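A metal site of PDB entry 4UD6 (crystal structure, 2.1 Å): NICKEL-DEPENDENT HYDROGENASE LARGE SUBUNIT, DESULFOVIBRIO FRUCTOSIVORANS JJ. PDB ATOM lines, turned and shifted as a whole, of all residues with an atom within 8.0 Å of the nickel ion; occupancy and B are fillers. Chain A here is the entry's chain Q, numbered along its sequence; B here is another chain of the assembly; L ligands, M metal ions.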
ATOM      1  N   GLU A  25      27.338  -8.356 -13.769  1.00  0.00           N
ATOM      2  CA  GLU A  25      25.922  -8.704 -13.782  1.00  0.00           C
ATOM      3  C   GLU A  25      25.177  -7.436 -13.388  1.00  0.00           C
ATOM      4  O   GLU A  25      25.534  -6.766 -12.395  1.00  0.00           O
ATOM      5  CB  GLU A  25      25.623  -9.809 -12.752  1.00  0.00           C
ATOM      6  CG  GLU A  25      24.222 -10.421 -12.896  1.00  0.00           C
ATOM      7  CD  GLU A  25      23.136  -9.425 -12.550  1.00  0.00           C
ATOM      8  OE1 GLU A  25      23.294  -8.718 -11.535  1.00  0.00           O
ATOM      9  OE2 GLU A  25      22.142  -9.293 -13.301  1.00  0.00           O
ATOM     10  N   GLN A  69      16.874 -17.641  -5.235  1.00  0.00           N
ATOM     11  CA  GLN A  69      17.952 -18.068  -6.150  1.00  0.00           C
ATOM     12  C   GLN A  69      17.990 -17.156  -7.392  1.00  0.00           C
ATOM     13  O   GLN A  69      19.051 -16.859  -7.915  1.00  0.00           O
ATOM     14  CB  GLN A  69      17.818 -19.531  -6.592  1.00  0.00           C
ATOM     15  CG  GLN A  69      19.067 -19.967  -7.354  1.00  0.00           C
ATOM     16  CD  GLN A  69      19.216 -21.454  -7.632  1.00  0.00           C
ATOM     17  OE1 GLN A  69      20.315 -21.874  -7.980  1.00  0.00           O
ATOM     18  NE2 GLN A  69      18.134 -22.232  -7.547  1.00  0.00           N
ATOM     19  N   ALA A  71      17.545 -14.059  -7.422  1.00  0.00           N
ATOM     20  CA  ALA A  71      18.336 -12.831  -7.218  1.00  0.00           C
ATOM     21  C   ALA A  71      19.474 -12.754  -8.227  1.00  0.00           C
ATOM     22  O   ALA A  71      19.845 -11.667  -8.664  1.00  0.00           O
ATOM     23  CB  ALA A  71      18.896 -12.730  -5.803  1.00  0.00           C
ATOM     24  N   CYS A  72      20.037 -13.903  -8.618  1.00  0.00           N
ATOM     25  CA  CYS A  72      21.175 -13.876  -9.499  1.00  0.00           C
ATOM     26  C   CYS A  72      21.439 -15.207 -10.197  1.00  0.00           C
ATOM     27  O   CYS A  72      21.395 -16.251  -9.561  1.00  0.00           O
ATOM     28  CB  CYS A  72      22.406 -13.443  -8.715  1.00  0.00           C
ATOM     29  SG  CYS A  72      23.818 -13.147  -9.802  1.00  0.00           S
ATOM     30  N   GLY A  73      21.749 -15.150 -11.502  1.00  0.00           N
ATOM     31  CA  GLY A  73      22.008 -16.321 -12.306  1.00  0.00           C
ATOM     32  C   GLY A  73      23.471 -16.476 -12.549  1.00  0.00           C
ATOM     33  O   GLY A  73      23.902 -17.463 -13.110  1.00  0.00           O
ATOM     34  N   VAL A  74      24.240 -15.461 -12.177  1.00  0.00           N
ATOM     35  CA  VAL A  74      25.698 -15.533 -12.271  1.00  0.00           C
ATOM     36  C   VAL A  74      26.232 -16.278 -11.037  1.00  0.00           C
ATOM     37  O   VAL A  74      26.835 -17.365 -11.179  1.00  0.00           O
ATOM     38  CB  VAL A  74      26.356 -14.135 -12.518  1.00  0.00           C
ATOM     39  CG1 VAL A  74      27.875 -14.258 -12.547  1.00  0.00           C
ATOM     40  CG2 VAL A  74      25.890 -13.582 -13.852  1.00  0.00           C
ATOM     41  N   CYS A  75      25.973 -15.735  -9.840  1.00  0.00           N
ATOM     42  CA  CYS A  75      26.110 -16.500  -8.618  1.00  0.00           C
ATOM     43  C   CYS A  75      24.843 -17.303  -8.405  1.00  0.00           C
ATOM     44  O   CYS A  75      24.150 -17.191  -7.372  1.00  0.00           O
ATOM     45  CB  CYS A  75      26.430 -15.614  -7.400  1.00  0.00           C
ATOM     46  SG  CYS A  75      25.160 -14.384  -6.997  1.00  0.00           S
ATOM     47  N   THR A  76      24.518 -18.122  -9.403  1.00  0.00           N
ATOM     48  CA  THR A  76      23.473 -19.097  -9.245  1.00  0.00           C
ATOM     49  C   THR A  76      23.818 -19.971  -8.041  1.00  0.00           C
ATOM     50  O   THR A  76      24.988 -19.982  -7.572  1.00  0.00           O
ATOM     51  CB  THR A  76      23.240 -19.942 -10.538  1.00  0.00           C
ATOM     52  OG1 THR A  76      22.014 -20.676 -10.396  1.00  0.00           O
ATOM     53  CG2 THR A  76      24.398 -20.880 -10.868  1.00  0.00           C
ATOM     54  N   VAL A  78      23.991 -19.887  -4.975  1.00  0.00           N
ATOM     55  CA  VAL A  78      24.346 -19.300  -3.654  1.00  0.00           C
ATOM     56  C   VAL A  78      23.130 -18.836  -2.839  1.00  0.00           C
ATOM     57  O   VAL A  78      23.093 -19.067  -1.609  1.00  0.00           O
ATOM     58  CB  VAL A  78      25.446 -18.217  -3.710  1.00  0.00           C
ATOM     59  CG1 VAL A  78      26.602 -18.662  -4.592  1.00  0.00           C
ATOM     60  CG2 VAL A  78      24.898 -16.859  -4.193  1.00  0.00           C
ATOM     61  N   HIS A  79      22.126 -18.234  -3.476  1.00  0.00           N
ATOM     62  CA  HIS A  79      20.955 -17.764  -2.726  1.00  0.00           C
ATOM     63  C   HIS A  79      20.030 -18.891  -2.308  1.00  0.00           C
ATOM     64  O   HIS A  79      19.460 -18.847  -1.201  1.00  0.00           O
ATOM     65  CB  HIS A  79      20.166 -16.704  -3.498  1.00  0.00           C
ATOM     66  CG  HIS A  79      20.910 -15.414  -3.675  1.00  0.00           C
ATOM     67  ND1 HIS A  79      20.996 -14.472  -2.662  1.00  0.00           N
ATOM     68  CD2 HIS A  79      21.587 -14.902  -4.725  1.00  0.00           C
ATOM     69  CE1 HIS A  79      21.702 -13.434  -3.088  1.00  0.00           C
ATOM     70  NE2 HIS A  79      22.089 -13.679  -4.327  1.00  0.00           N
ATOM     71  N   GLN A 110      30.720 -23.760  -7.821  1.00  0.00           N
ATOM     72  CA  GLN A 110      30.297 -22.411  -8.205  1.00  0.00           C
ATOM     73  C   GLN A 110      31.502 -21.463  -8.241  1.00  0.00           C
ATOM     74  O   GLN A 110      31.713 -20.760  -9.236  1.00  0.00           O
ATOM     75  CB  GLN A 110      29.180 -21.892  -7.273  1.00  0.00           C
ATOM     76  CG  GLN A 110      28.729 -20.463  -7.529  1.00  0.00           C
ATOM     77  CD  GLN A 110      28.218 -20.251  -8.959  1.00  0.00           C
ATOM     78  OE1 GLN A 110      27.752 -21.185  -9.614  1.00  0.00           O
ATOM     79  NE2 GLN A 110      28.310 -18.997  -9.437  1.00  0.00           N
ATOM     80  N   ASP A 114      32.504 -19.459 -11.548  1.00  0.00           N
ATOM     81  CA  ASP A 114      32.258 -18.022 -11.400  1.00  0.00           C
ATOM     82  C   ASP A 114      33.559 -17.273 -11.613  1.00  0.00           C
ATOM     83  O   ASP A 114      33.618 -16.392 -12.456  1.00  0.00           O
ATOM     84  CB  ASP A 114      31.602 -17.732 -10.025  1.00  0.00           C
ATOM     85  CG  ASP A 114      30.826 -16.404  -9.987  1.00  0.00           C
ATOM     86  OD1 ASP A 114      31.211 -15.444 -10.689  1.00  0.00           O
ATOM     87  OD2 ASP A 114      29.837 -16.323  -9.218  1.00  0.00           O
ATOM     88  N   ALA A 474      29.694 -16.402  -0.613  1.00  0.00           N
ATOM     89  CA  ALA A 474      29.509 -16.594  -2.021  1.00  0.00           C
ATOM     90  C   ALA A 474      30.770 -16.127  -2.732  1.00  0.00           C
ATOM     91  O   ALA A 474      31.611 -15.475  -2.116  1.00  0.00           O
ATOM     92  CB  ALA A 474      28.312 -15.817  -2.492  1.00  0.00           C
ATOM     93  N   PRO A 475      30.909 -16.454  -4.044  1.00  0.00           N
ATOM     94  CA  PRO A 475      32.087 -15.994  -4.774  1.00  0.00           C
ATOM     95  C   PRO A 475      32.395 -14.505  -4.618  1.00  0.00           C
ATOM     96  O   PRO A 475      33.566 -14.126  -4.661  1.00  0.00           O
ATOM     97  CB  PRO A 475      31.732 -16.319  -6.224  1.00  0.00           C
ATOM     98  CG  PRO A 475      30.829 -17.521  -6.108  1.00  0.00           C
ATOM     99  CD  PRO A 475      30.020 -17.270  -4.887  1.00  0.00           C
ATOM    100  N   ARG A 476      31.377 -13.675  -4.394  1.00  0.00           N
ATOM    101  CA  ARG A 476      31.572 -12.229  -4.229  1.00  0.00           C
ATOM    102  C   ARG A 476      31.616 -11.804  -2.755  1.00  0.00           C
ATOM    103  O   ARG A 476      31.863 -10.640  -2.448  1.00  0.00           O
ATOM    104  CB  ARG A 476      30.483 -11.447  -4.968  1.00  0.00           C
ATOM    105  CG  ARG A 476      30.698 -11.330  -6.470  1.00  0.00           C
ATOM    106  CD  ARG A 476      29.416 -11.140  -7.309  1.00  0.00           C
ATOM    107  NE  ARG A 476      29.748 -11.447  -8.717  1.00  0.00           N
ATOM    108  CZ  ARG A 476      29.773 -12.689  -9.200  1.00  0.00           C
ATOM    109  NH1 ARG A 476      29.386 -13.714  -8.442  1.00  0.00           N
ATOM    110  NH2 ARG A 476      30.157 -12.893 -10.435  1.00  0.00           N
ATOM    111  N   VAL A 497      23.537  -8.861   0.775  1.00  0.00           N
ATOM    112  CA  VAL A 497      24.221  -9.613  -0.252  1.00  0.00           C
ATOM    113  C   VAL A 497      25.574  -8.961  -0.443  1.00  0.00           C
ATOM    114  O   VAL A 497      25.707  -7.770  -0.205  1.00  0.00           O
ATOM    115  CB  VAL A 497      23.372  -9.653  -1.529  1.00  0.00           C
ATOM    116  CG1 VAL A 497      23.938 -10.660  -2.554  1.00  0.00           C
ATOM    117  CG2 VAL A 497      21.952 -10.078  -1.154  1.00  0.00           C
ATOM    118  N   PRO A 498      26.593  -9.751  -0.843  1.00  0.00           N
ATOM    119  CA  PRO A 498      27.927  -9.141  -0.871  1.00  0.00           C
ATOM    120  C   PRO A 498      28.034  -7.849  -1.687  1.00  0.00           C
ATOM    121  O   PRO A 498      28.642  -6.900  -1.216  1.00  0.00           O
ATOM    122  CB  PRO A 498      28.836 -10.225  -1.465  1.00  0.00           C
ATOM    123  CG  PRO A 498      27.950 -11.361  -1.865  1.00  0.00           C
ATOM    124  CD  PRO A 498      26.681 -11.219  -1.046  1.00  0.00           C
ATOM    125  N   SER A 499      27.454  -7.815  -2.881  1.00  0.00           N
ATOM    126  CA  SER A 499      27.493  -6.577  -3.681  1.00  0.00           C
ATOM    127  C   SER A 499      26.710  -5.431  -3.021  1.00  0.00           C
ATOM    128  O   SER A 499      26.950  -4.286  -3.350  1.00  0.00           O
ATOM    129  CB  SER A 499      27.019  -6.795  -5.133  1.00  0.00           C
ATOM    130  OG  SER A 499      27.918  -7.643  -5.850  1.00  0.00           O
ATOM    131  N   ASP A 541      33.925  -7.303  -8.743  1.00  0.00           N
ATOM    132  CA  ASP A 541      33.059  -8.344  -9.352  1.00  0.00           C
ATOM    133  C   ASP A 541      31.580  -8.011  -9.077  1.00  0.00           C
ATOM    134  O   ASP A 541      30.871  -8.756  -8.397  1.00  0.00           O
ATOM    135  CB  ASP A 541      33.459  -9.744  -8.814  1.00  0.00           C
ATOM    136  CG  ASP A 541      32.761 -10.888  -9.522  1.00  0.00           C
ATOM    137  OD1 ASP A 541      31.918 -10.674 -10.459  1.00  0.00           O
ATOM    138  OD2 ASP A 541      33.055 -12.061  -9.130  1.00  0.00           O
ATOM    139  N   PRO A 542      31.120  -6.855  -9.590  1.00  0.00           N
ATOM    140  CA  PRO A 542      29.803  -6.385  -9.161  1.00  0.00           C
ATOM    141  C   PRO A 542      28.661  -7.277  -9.636  1.00  0.00           C
ATOM    142  O   PRO A 542      28.722  -7.827 -10.757  1.00  0.00           O
ATOM    143  CB  PRO A 542      29.707  -4.985  -9.809  1.00  0.00           C
ATOM    144  CG  PRO A 542      31.132  -4.568  -9.999  1.00  0.00           C
ATOM    145  CD  PRO A 542      31.838  -5.858 -10.392  1.00  0.00           C
ATOM    146  N   CSO A 543      27.671  -7.450  -8.773  1.00  0.00           N
ATOM    147  CA  CSO A 543      26.432  -8.167  -9.107  1.00  0.00           C
ATOM    148  CB  CSO A 543      26.454  -9.511  -8.421  1.00  0.00           C
ATOM    149  SG  CSO A 543      25.544 -10.688  -9.377  1.00  0.00           S
ATOM    150  C   CSO A 543      25.259  -7.321  -8.618  1.00  0.00           C
ATOM    151  O   CSO A 543      24.942  -7.294  -7.412  1.00  0.00           O
ATOM    152  OD  CSO A 543      23.913 -10.131  -9.385  1.00  0.00           O
ATOM    153  N   ILE A 544      24.631  -6.598  -9.534  1.00  0.00           N
ATOM    154  CA  ILE A 544      23.709  -5.517  -9.086  1.00  0.00           C
ATOM    155  C   ILE A 544      22.343  -6.119  -8.800  1.00  0.00           C
ATOM    156  O   ILE A 544      21.610  -5.628  -7.946  1.00  0.00           O
ATOM    157  CB  ILE A 544      23.649  -4.354 -10.099  1.00  0.00           C
ATOM    158  CG1 ILE A 544      25.053  -3.909 -10.487  1.00  0.00           C
ATOM    159  CG2 ILE A 544      22.792  -3.188  -9.569  1.00  0.00           C
ATOM    160  CD1 ILE A 544      25.963  -3.519  -9.324  1.00  0.00           C
ATOM    161  N   ALA A 545      22.020  -7.204  -9.505  1.00  0.00           N
ATOM    162  CA  ALA A 545      20.759  -7.916  -9.221  1.00  0.00           C
ATOM    163  C   ALA A 545      20.885  -8.552  -7.831  1.00  0.00           C
ATOM    164  O   ALA A 545      19.915  -8.591  -7.068  1.00  0.00           O
ATOM    165  CB  ALA A 545      20.458  -8.953 -10.305  1.00  0.00           C
ATOM    166  N   CYS A 546      22.080  -9.031  -7.509  1.00  0.00           N
ATOM    167  CA  CYS A 546      22.371  -9.500  -6.144  1.00  0.00           C
ATOM    168  C   CYS A 546      22.241  -8.340  -5.137  1.00  0.00           C
ATOM    169  O   CYS A 546      21.567  -8.456  -4.103  1.00  0.00           O
ATOM    170  CB  CYS A 546      23.777 -10.083  -6.055  1.00  0.00           C
ATOM    171  SG  CYS A 546      23.842 -11.858  -6.236  1.00  0.00           S
ATOM    172  N   GLY A 547      22.892  -7.227  -5.442  1.00  0.00           N
ATOM    173  CA  GLY A 547      22.991  -6.118  -4.500  1.00  0.00           C
ATOM    174  C   GLY A 547      21.643  -5.550  -4.117  1.00  0.00           C
ATOM    175  O   GLY A 547      21.398  -5.294  -2.944  1.00  0.00           O
ATOM    176  N   CYS B  17      18.017 -11.686 -13.938  1.00  0.00           N
ATOM    177  CA  CYS B  17      19.073 -12.132 -13.029  1.00  0.00           C
ATOM    178  C   CYS B  17      20.360 -12.518 -13.778  1.00  0.00           C
ATOM    179  O   CYS B  17      21.366 -12.818 -13.161  1.00  0.00           O
ATOM    180  CB  CYS B  17      18.580 -13.322 -12.190  1.00  0.00           C
ATOM    181  SG  CYS B  17      18.598 -14.923 -13.065  1.00  0.00           S
ATOM    182  N   THR B  18      20.293 -12.516 -15.108  1.00  0.00           N
ATOM    183  CA  THR B  18      21.420 -12.868 -16.014  1.00  0.00           C
ATOM    184  C   THR B  18      21.644 -14.377 -16.104  1.00  0.00           C
ATOM    185  O   THR B  18      22.611 -14.843 -16.738  1.00  0.00           O
ATOM    186  CB  THR B  18      22.700 -12.080 -15.667  1.00  0.00           C
ATOM    187  OG1 THR B  18      22.371 -10.685 -15.481  1.00  0.00           O
ATOM    188  CG2 THR B  18      23.766 -12.213 -16.772  1.00  0.00           C
HETATM  189 FE1  LIG L   1      25.942 -12.692  -5.745  1.00  0.00          FE
HETATM  190  C1  LIG L   1      26.568 -10.979  -5.163  1.00  0.00           C
HETATM  191  N1  LIG L   1      26.950  -9.943  -4.781  1.00  0.00           N
HETATM  192  C2  LIG L   1      27.628 -13.533  -5.491  1.00  0.00           C
HETATM  193  N2  LIG L   1      28.639 -14.093  -5.364  1.00  0.00           N
HETATM  194  C3  LIG L   1      25.601 -13.209  -4.126  1.00  0.00           C
HETATM  195  O1  LIG L   1      25.394 -13.572  -3.080  1.00  0.00           O
HETATM  196 NI    NI M   1      25.274 -12.561  -8.240  1.00  0.00          NI
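An iron atom (FE1) of the ligand is bound by the side-chain sulfur of Cys 75, at 2.2 Å. The side-chain sulfur (SG) of Cys 546 is bound to an iron atom (FE1) of the ligand (2.3 Å). The backbone NH (N) of Arg 476 sits at hydrogen-bond distance from a nitrogen (N2) of the ligand (2.9 Å). The guanidinium group of Arg 476 lies within hydrogen-bond range of a nitrogen (N2) of the ligand (3.2 Å). The backbone NH of Ser 499 lies within hydrogen-bond range of a nitrogen (N1) of the ligand. The side-chain hydroxyl (OG) of Ser 499 is in hydrogen-bond range of a nitrogen (N1) of the ligand, 2.7 Å away.
OD of CSO 543 sits at hydrogen-bond distance from OE1 of Glu 25 (2.6 Å). OD of CSO 543 sits close to the backbone NH (N) of Ala 545, at 3.5 Å. N of CSO 543 is in hydrogen-bond range of OG of Ser 499 (2.9 Å). N of Val 74 sits close to SG of Cys 72, at 3.3 Å. The side-chain sulfur (SG) of Cys 546 lies close to a ring nitrogen (NE2) of His 79 (3.2 Å).
SG of CSO 543 binds the nickel ion. The nickel ion is bound by SG of Cys 75, at 2.2 Å. The nickel ion is bound by the side-chain sulfur (SG) of Cys 72 (2.2 Å). The nickel ion is bound by the side-chain sulfur (SG) of Cys 546. The nickel ion has four donor atoms within binding distance.
Four residues have an atom within 4 Å of the nickel ion: Cys 72, Cys 75, CSO 543 and Cys 546. Along chain A the residues within 4 Å of the nickel ion span positions 72 to 546.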
